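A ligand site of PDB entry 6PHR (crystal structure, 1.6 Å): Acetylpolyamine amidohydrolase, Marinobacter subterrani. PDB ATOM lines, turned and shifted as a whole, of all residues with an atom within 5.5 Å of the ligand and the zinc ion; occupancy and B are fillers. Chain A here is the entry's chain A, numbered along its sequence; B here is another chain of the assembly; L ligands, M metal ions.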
ATOM      1  N   GLU A  22       7.940   6.070 -22.106  1.00  0.00           N
ATOM      2  CA  GLU A  22       6.845   6.384 -23.027  1.00  0.00           C
ATOM      3  C   GLU A  22       7.348   6.174 -24.454  1.00  0.00           C
ATOM      4  O   GLU A  22       8.395   6.720 -24.832  1.00  0.00           O
ATOM      5  CB  GLU A  22       6.342   7.823 -22.849  1.00  0.00           C
ATOM      6  CG  GLU A  22       5.474   8.290 -24.002  1.00  0.00           C
ATOM      7  CD  GLU A  22       4.800   9.622 -23.750  1.00  0.00           C
ATOM      8  OE1 GLU A  22       4.858  10.116 -22.596  1.00  0.00           O
ATOM      9  OE2 GLU A  22       4.230  10.165 -24.716  1.00  0.00           O
ATOM     10  N   LEU A  23       6.638   5.373 -25.236  1.00  0.00           N
ATOM     11  CA  LEU A  23       6.974   5.220 -26.647  1.00  0.00           C
ATOM     12  C   LEU A  23       6.663   6.507 -27.417  1.00  0.00           C
ATOM     13  O   LEU A  23       5.524   6.984 -27.404  1.00  0.00           O
ATOM     14  CB  LEU A  23       6.192   4.046 -27.248  1.00  0.00           C
ATOM     15  CG  LEU A  23       6.399   3.879 -28.760  1.00  0.00           C
ATOM     16  CD1 LEU A  23       7.823   3.446 -29.058  1.00  0.00           C
ATOM     17  CD2 LEU A  23       5.413   2.887 -29.357  1.00  0.00           C
ATOM     18  N   ASP A  24       7.685   7.075 -28.060  1.00  0.00           N
ATOM     19  CA  ASP A  24       7.522   8.337 -28.767  1.00  0.00           C
ATOM     20  C   ASP A  24       8.522   8.380 -29.911  1.00  0.00           C
ATOM     21  O   ASP A  24       9.727   8.251 -29.680  1.00  0.00           O
ATOM     22  CB  ASP A  24       7.730   9.527 -27.802  1.00  0.00           C
ATOM     23  CG  ASP A  24       7.488  10.888 -28.461  1.00  0.00           C
ATOM     24  OD1 ASP A  24       8.445  11.478 -29.006  1.00  0.00           O
ATOM     25  OD2 ASP A  24       6.340  11.387 -28.399  1.00  0.00           O
ATOM     26  N   GLY A  25       8.029   8.518 -31.145  1.00  0.00           N
ATOM     27  CA  GLY A  25       8.936   8.630 -32.274  1.00  0.00           C
ATOM     28  C   GLY A  25       9.898   7.473 -32.433  1.00  0.00           C
ATOM     29  O   GLY A  25      11.031   7.679 -32.855  1.00  0.00           O
ATOM     30  N   HIS A  32       5.645  12.258 -20.678  1.00  0.00           N
ATOM     31  CA  HIS A  32       5.158  13.634 -20.554  1.00  0.00           C
ATOM     32  C   HIS A  32       4.230  13.804 -19.361  1.00  0.00           C
ATOM     33  O   HIS A  32       4.209  14.883 -18.743  1.00  0.00           O
ATOM     34  CB  HIS A  32       4.406  14.036 -21.818  1.00  0.00           C
ATOM     35  CG  HIS A  32       5.271  14.255 -23.018  1.00  0.00           C
ATOM     36  ND1 HIS A  32       6.087  15.365 -23.149  1.00  0.00           N
ATOM     37  CD2 HIS A  32       5.427  13.542 -24.152  1.00  0.00           C
ATOM     38  CE1 HIS A  32       6.709  15.319 -24.312  1.00  0.00           C
ATOM     39  NE2 HIS A  32       6.334  14.222 -24.938  1.00  0.00           N
ATOM     40  N   ASP A 122       1.672   4.518 -26.015  1.00  0.00           N
ATOM     41  CA  ASP A 122       2.414   5.560 -25.305  1.00  0.00           C
ATOM     42  C   ASP A 122       2.012   5.688 -23.840  1.00  0.00           C
ATOM     43  O   ASP A 122       2.487   6.614 -23.163  1.00  0.00           O
ATOM     44  CB  ASP A 122       2.257   6.901 -26.025  1.00  0.00           C
ATOM     45  CG  ASP A 122       0.815   7.350 -26.125  1.00  0.00           C
ATOM     46  OD1 ASP A 122      -0.063   6.639 -25.626  1.00  0.00           O
ATOM     47  OD2 ASP A 122       0.572   8.443 -26.682  1.00  0.00           O
ATOM     48  N   PRO A 161      -5.100  11.790 -16.106  1.00  0.00           N
ATOM     49  CA  PRO A 161      -6.292  12.357 -16.754  1.00  0.00           C
ATOM     50  C   PRO A 161      -7.243  11.268 -17.240  1.00  0.00           C
ATOM     51  O   PRO A 161      -6.955  10.063 -17.113  1.00  0.00           O
ATOM     52  CB  PRO A 161      -5.713  13.153 -17.925  1.00  0.00           C
ATOM     53  CG  PRO A 161      -4.466  12.333 -18.292  1.00  0.00           C
ATOM     54  CD  PRO A 161      -3.905  11.891 -16.962  1.00  0.00           C
ATOM     55  N   HIS A 163      -9.988  11.899 -20.265  1.00  0.00           N
ATOM     56  CA  HIS A 163     -10.968  12.111 -21.332  1.00  0.00           C
ATOM     57  C   HIS A 163     -10.752  11.220 -22.551  1.00  0.00           C
ATOM     58  O   HIS A 163     -11.663  11.117 -23.386  1.00  0.00           O
ATOM     59  CB  HIS A 163     -11.017  13.594 -21.732  1.00  0.00           C
ATOM     60  CG  HIS A 163      -9.784  14.090 -22.428  1.00  0.00           C
ATOM     61  ND1 HIS A 163      -9.825  15.078 -23.389  1.00  0.00           N
ATOM     62  CD2 HIS A 163      -8.481  13.745 -22.291  1.00  0.00           C
ATOM     63  CE1 HIS A 163      -8.605  15.301 -23.837  1.00  0.00           C
ATOM     64  NE2 HIS A 163      -7.765  14.528 -23.176  1.00  0.00           N
ATOM     65  N   HIS A 164      -9.606  10.527 -22.665  1.00  0.00           N
ATOM     66  CA  HIS A 164      -9.367   9.611 -23.781  1.00  0.00           C
ATOM     67  C   HIS A 164      -9.801   8.170 -23.507  1.00  0.00           C
ATOM     68  O   HIS A 164      -9.805   7.365 -24.439  1.00  0.00           O
ATOM     69  CB  HIS A 164      -7.884   9.586 -24.151  1.00  0.00           C
ATOM     70  CG  HIS A 164      -7.403  10.869 -24.736  1.00  0.00           C
ATOM     71  ND1 HIS A 164      -8.055  11.513 -25.766  1.00  0.00           N
ATOM     72  CD2 HIS A 164      -6.351  11.661 -24.395  1.00  0.00           C
ATOM     73  CE1 HIS A 164      -7.397  12.613 -26.075  1.00  0.00           C
ATOM     74  NE2 HIS A 164      -6.373  12.734 -25.249  1.00  0.00           N
ATOM     75  N   GLY A 172      -3.922   7.485 -24.387  1.00  0.00           N
ATOM     76  CA  GLY A 172      -3.766   8.928 -24.251  1.00  0.00           C
ATOM     77  C   GLY A 172      -3.503   9.329 -22.817  1.00  0.00           C
ATOM     78  O   GLY A 172      -3.947  10.396 -22.367  1.00  0.00           O
ATOM     79  N   TYR A 173      -2.775   8.485 -22.097  1.00  0.00           N
ATOM     80  CA  TYR A 173      -2.392   8.696 -20.705  1.00  0.00           C
ATOM     81  C   TYR A 173      -3.550   8.521 -19.731  1.00  0.00           C
ATOM     82  O   TYR A 173      -3.397   8.819 -18.541  1.00  0.00           O
ATOM     83  CB  TYR A 173      -1.767  10.089 -20.469  1.00  0.00           C
ATOM     84  CG  TYR A 173      -0.700  10.541 -21.450  1.00  0.00           C
ATOM     85  CD1 TYR A 173       0.091   9.627 -22.141  1.00  0.00           C
ATOM     86  CD2 TYR A 173      -0.482  11.897 -21.658  1.00  0.00           C
ATOM     87  CE1 TYR A 173       1.075  10.058 -23.034  1.00  0.00           C
ATOM     88  CE2 TYR A 173       0.499  12.339 -22.542  1.00  0.00           C
ATOM     89  CZ  TYR A 173       1.274  11.419 -23.219  1.00  0.00           C
ATOM     90  OH  TYR A 173       2.233  11.862 -24.099  1.00  0.00           O
ATOM     91  N   CYS A 174      -4.693   8.020 -20.194  1.00  0.00           N
ATOM     92  CA  CYS A 174      -5.934   7.957 -19.419  1.00  0.00           C
ATOM     93  C   CYS A 174      -6.395   6.522 -19.203  1.00  0.00           C
ATOM     94  O   CYS A 174      -6.241   5.661 -20.090  1.00  0.00           O
ATOM     95  CB  CYS A 174      -7.069   8.667 -20.128  1.00  0.00           C
ATOM     96  SG  CYS A 174      -6.752  10.382 -20.579  1.00  0.00           S
ATOM     97  N   ASP A 200      -9.547  20.710 -23.576  1.00  0.00           N
ATOM     98  CA  ASP A 200      -8.230  20.164 -23.831  1.00  0.00           C
ATOM     99  C   ASP A 200      -7.925  20.188 -25.324  1.00  0.00           C
ATOM    100  O   ASP A 200      -8.818  20.115 -26.167  1.00  0.00           O
ATOM    101  CB  ASP A 200      -8.179  18.728 -23.274  1.00  0.00           C
ATOM    102  CG  ASP A 200      -6.814  18.059 -23.406  1.00  0.00           C
ATOM    103  OD1 ASP A 200      -6.451  17.599 -24.508  1.00  0.00           O
ATOM    104  OD2 ASP A 200      -6.099  17.962 -22.397  1.00  0.00           O
ATOM    105  N   PHE A 201      -6.633  20.331 -25.659  1.00  0.00           N
ATOM    106  CA  PHE A 201      -6.248  20.422 -27.062  1.00  0.00           C
ATOM    107  C   PHE A 201      -6.684  19.185 -27.842  1.00  0.00           C
ATOM    108  O   PHE A 201      -7.004  19.286 -29.025  1.00  0.00           O
ATOM    109  CB  PHE A 201      -4.723  20.602 -27.183  1.00  0.00           C
ATOM    110  CG  PHE A 201      -4.181  20.368 -28.582  1.00  0.00           C
ATOM    111  CD1 PHE A 201      -4.244  21.379 -29.544  1.00  0.00           C
ATOM    112  CD2 PHE A 201      -3.621  19.141 -28.934  1.00  0.00           C
ATOM    113  CE1 PHE A 201      -3.770  21.191 -30.806  1.00  0.00           C
ATOM    114  CE2 PHE A 201      -3.134  18.934 -30.227  1.00  0.00           C
ATOM    115  CZ  PHE A 201      -3.207  19.976 -31.171  1.00  0.00           C
ATOM    116  N   HIS A 202      -6.686  18.007 -27.203  1.00  0.00           N
ATOM    117  CA  HIS A 202      -7.021  16.778 -27.917  1.00  0.00           C
ATOM    118  C   HIS A 202      -8.509  16.481 -27.816  1.00  0.00           C
ATOM    119  O   HIS A 202      -9.183  16.905 -26.875  1.00  0.00           O
ATOM    120  CB  HIS A 202      -6.215  15.605 -27.354  1.00  0.00           C
ATOM    121  CG  HIS A 202      -4.735  15.812 -27.420  1.00  0.00           C
ATOM    122  ND1 HIS A 202      -4.030  16.441 -26.407  1.00  0.00           N
ATOM    123  CD2 HIS A 202      -3.843  15.574 -28.413  1.00  0.00           C
ATOM    124  CE1 HIS A 202      -2.767  16.557 -26.774  1.00  0.00           C
ATOM    125  NE2 HIS A 202      -2.626  16.041 -27.987  1.00  0.00           N
ATOM    126  N   PHE A 230      -3.345  13.228 -32.648  1.00  0.00           N
ATOM    127  CA  PHE A 230      -4.058  12.313 -31.765  1.00  0.00           C
ATOM    128  C   PHE A 230      -5.397  12.918 -31.342  1.00  0.00           C
ATOM    129  O   PHE A 230      -5.454  14.104 -30.970  1.00  0.00           O
ATOM    130  CB  PHE A 230      -3.172  12.036 -30.551  1.00  0.00           C
ATOM    131  CG  PHE A 230      -3.772  11.093 -29.569  1.00  0.00           C
ATOM    132  CD1 PHE A 230      -3.614   9.705 -29.742  1.00  0.00           C
ATOM    133  CD2 PHE A 230      -4.451  11.562 -28.460  1.00  0.00           C
ATOM    134  CE1 PHE A 230      -4.157   8.837 -28.852  1.00  0.00           C
ATOM    135  CE2 PHE A 230      -5.001  10.669 -27.555  1.00  0.00           C
ATOM    136  CZ  PHE A 230      -4.849   9.311 -27.742  1.00  0.00           C
ATOM    137  N   ASP A 289      -2.996  22.115 -22.512  1.00  0.00           N
ATOM    138  CA  ASP A 289      -2.081  21.889 -23.623  1.00  0.00           C
ATOM    139  C   ASP A 289      -2.492  22.661 -24.873  1.00  0.00           C
ATOM    140  O   ASP A 289      -1.936  22.438 -25.938  1.00  0.00           O
ATOM    141  CB  ASP A 289      -1.903  20.368 -23.922  1.00  0.00           C
ATOM    142  CG  ASP A 289      -3.211  19.558 -23.945  1.00  0.00           C
ATOM    143  OD1 ASP A 289      -4.312  20.145 -23.894  1.00  0.00           O
ATOM    144  OD2 ASP A 289      -3.132  18.283 -24.041  1.00  0.00           O
ATOM    145  N   ILE A 296       3.320  19.094 -27.129  1.00  0.00           N
ATOM    146  CA  ILE A 296       2.669  18.085 -27.960  1.00  0.00           C
ATOM    147  C   ILE A 296       1.353  18.636 -28.494  1.00  0.00           C
ATOM    148  O   ILE A 296       0.362  17.910 -28.630  1.00  0.00           O
ATOM    149  CB  ILE A 296       2.467  16.768 -27.198  1.00  0.00           C
ATOM    150  CG1 ILE A 296       1.620  16.959 -25.950  1.00  0.00           C
ATOM    151  CG2 ILE A 296       3.823  16.146 -26.824  1.00  0.00           C
ATOM    152  CD1 ILE A 296       1.509  15.668 -25.124  1.00  0.00           C
ATOM    153  N   GLU A 325      -7.262  17.563 -17.225  1.00  0.00           N
ATOM    154  CA  GLU A 325      -6.807  16.631 -18.260  1.00  0.00           C
ATOM    155  C   GLU A 325      -5.330  16.852 -18.563  1.00  0.00           C
ATOM    156  O   GLU A 325      -4.492  16.671 -17.673  1.00  0.00           O
ATOM    157  CB  GLU A 325      -7.679  16.757 -19.514  1.00  0.00           C
ATOM    158  CG  GLU A 325      -9.190  16.618 -19.249  1.00  0.00           C
ATOM    159  CD  GLU A 325      -9.611  15.220 -18.778  1.00  0.00           C
ATOM    160  OE1 GLU A 325      -8.905  14.234 -19.046  1.00  0.00           O
ATOM    161  OE2 GLU A 325     -10.687  15.112 -18.155  1.00  0.00           O
ATOM    162  N   GLY A 326      -4.994  17.287 -19.796  1.00  0.00           N
ATOM    163  CA  GLY A 326      -3.610  17.489 -20.205  1.00  0.00           C
ATOM    164  C   GLY A 326      -3.041  18.882 -19.920  1.00  0.00           C
ATOM    165  O   GLY A 326      -3.666  19.725 -19.275  1.00  0.00           O
ATOM    166  N   GLY A 327      -1.836  19.124 -20.450  1.00  0.00           N
ATOM    167  CA  GLY A 327      -1.001  20.306 -20.196  1.00  0.00           C
ATOM    168  C   GLY A 327       0.405  19.838 -19.842  1.00  0.00           C
ATOM    169  O   GLY A 327       0.582  19.253 -18.768  1.00  0.00           O
ATOM    170  N   TYR A 328       1.405  20.068 -20.717  1.00  0.00           N
ATOM    171  CA  TYR A 328       2.682  19.366 -20.605  1.00  0.00           C
ATOM    172  C   TYR A 328       3.917  20.270 -20.626  1.00  0.00           C
ATOM    173  O   TYR A 328       5.046  19.749 -20.569  1.00  0.00           O
ATOM    174  CB  TYR A 328       2.789  18.300 -21.719  1.00  0.00           C
ATOM    175  CG  TYR A 328       1.633  17.353 -21.581  1.00  0.00           C
ATOM    176  CD1 TYR A 328       0.485  17.510 -22.358  1.00  0.00           C
ATOM    177  CD2 TYR A 328       1.624  16.400 -20.576  1.00  0.00           C
ATOM    178  CE1 TYR A 328      -0.635  16.649 -22.187  1.00  0.00           C
ATOM    179  CE2 TYR A 328       0.527  15.551 -20.380  1.00  0.00           C
ATOM    180  CZ  TYR A 328      -0.600  15.694 -21.189  1.00  0.00           C
ATOM    181  OH  TYR A 328      -1.673  14.868 -20.990  1.00  0.00           O
ATOM    182  N   THR B  95       2.512   4.321 -32.776  1.00  0.00           N
ATOM    183  CA  THR B  95       2.217   4.690 -31.405  1.00  0.00           C
ATOM    184  C   THR B  95       0.729   4.632 -31.073  1.00  0.00           C
ATOM    185  O   THR B  95       0.371   4.435 -29.914  1.00  0.00           O
ATOM    186  CB  THR B  95       2.720   6.099 -31.081  1.00  0.00           C
ATOM    187  OG1 THR B  95       3.980   6.357 -31.735  1.00  0.00           O
ATOM    188  CG2 THR B  95       2.886   6.285 -29.560  1.00  0.00           C
ATOM    189  N   PHE B  96      -0.130   4.828 -32.075  1.00  0.00           N
ATOM    190  CA  PHE B  96      -1.581   4.886 -31.899  1.00  0.00           C
ATOM    191  C   PHE B  96      -2.224   4.133 -33.036  1.00  0.00           C
ATOM    192  O   PHE B  96      -1.660   4.055 -34.125  1.00  0.00           O
ATOM    193  CB  PHE B  96      -2.136   6.327 -31.948  1.00  0.00           C
ATOM    194  CG  PHE B  96      -1.159   7.387 -31.554  1.00  0.00           C
ATOM    195  CD1 PHE B  96      -0.793   7.529 -30.230  1.00  0.00           C
ATOM    196  CD2 PHE B  96      -0.649   8.280 -32.494  1.00  0.00           C
ATOM    197  CE1 PHE B  96       0.081   8.518 -29.840  1.00  0.00           C
ATOM    198  CE2 PHE B  96       0.226   9.271 -32.094  1.00  0.00           C
ATOM    199  CZ  PHE B  96       0.597   9.383 -30.756  1.00  0.00           C
HETATM  200  C1  LIG L   1       3.043   9.974 -27.869  1.00  0.00           C
HETATM  201  C2  LIG L   1       2.740  11.448 -27.574  1.00  0.00           C
HETATM  202  C3  LIG L   1       1.249  11.657 -27.773  1.00  0.00           C
HETATM  203  C4  LIG L   1      -0.941  11.142 -26.997  1.00  0.00           C
HETATM  204  C5  LIG L   1      -1.566  12.481 -26.662  1.00  0.00           C
HETATM  205  C6  LIG L   1      -1.991  12.453 -25.211  1.00  0.00           C
HETATM  206  C7  LIG L   1      -2.849  13.683 -24.885  1.00  0.00           C
HETATM  207  C8  LIG L   1      -3.301  13.486 -23.445  1.00  0.00           C
HETATM  208  N1  LIG L   1       4.353   9.607 -27.342  1.00  0.00           N
HETATM  209  N2  LIG L   1       0.481  11.099 -26.669  1.00  0.00           N
HETATM  210  S1  LIG L   1      -4.310  14.858 -22.810  1.00  0.00           S
HETATM  211 ZN    ZN M   1      -4.492  16.815 -24.264  1.00  0.00          ZN
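Along chain A the residues within 4 Å of the zinc ion span positions 200 to 289.
OD2 of Asp 122 lies within salt-bridge range of N2 of the ligand (2.7 Å). The side-chain hydroxyl of Tyr 173 is in hydrogen-bond range of a nitrogen (N2) of the ligand. OH of Tyr 328 sits close to S1 of the ligand, at 3.2 Å. The side-chain carboxylate of Asp 24 lies within salt-bridge range of a nitrogen (N1) of the ligand, 2.9 Å away. S1 of the ligand lies close to NE2 of His 163 (3.5 Å). A nitrogen (N1) of the ligand lies within hydrogen-bond range of the backbone carbonyl oxygen (O) of Leu 23, at 2.9 Å. OE2 of Glu 22 is in salt-bridge range of N1 of the ligand (2.7 Å).
Merely in contact with the ligand: Gly 172 (3.3 Å), Phe 230 (3.5 Å), His 164 (3.6 Å), Gly 326 (3.8 Å) and Phe 96 of chain B (3.8 Å). Hydrophobic or aromatic side chains that line the ligand: His 164, Tyr 173, His 202, Phe 230 and Phe 96 of chain B. Of the 24 residues printed, 15 come within 4 Å of the ligand.
N of His 163 sits at hydrogen-bond distance from OE1 of Glu 325 (2.8 Å). N of His 164 lies within hydrogen-bond range of SG of Cys 174, 3.5 Å away. N of Phe 201 sits at hydrogen-bond distance from OD1 of Asp 289 (2.9 Å). OH of Tyr 173 is in hydrogen-bond range of OE2 of Glu 22, at 2.7 Å. A ring nitrogen (NE2) of His 163 is in hydrogen-bond range of a ring nitrogen (NE2) of His 164, at 3.1 Å. N of His 163 is in hydrogen-bond range of SG of Cys 174 (3.6 Å). The backbone carbonyl oxygen (O) of Gly 172 sits at hydrogen-bond distance from the side-chain sulfur (SG) of Cys 174 (3.3 Å). The side-chain carboxylate (OE1) of Glu 22 is in hydrogen-bond range of the backbone NH (N) of His 32 (3.0 Å).
OD2 of Asp 289 binds the zinc ion. OD1 of Asp 200 is bound to the zinc ion (2.1 Å). The zinc ion is bound by ND1 of His 202 (2.2 Å). S1 of the ligand binds the zinc ion, 2.4 Å away. Slightly farther from the zinc ion lies the side-chain carboxylate (OD2) of Asp 200 (2.7 Å).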
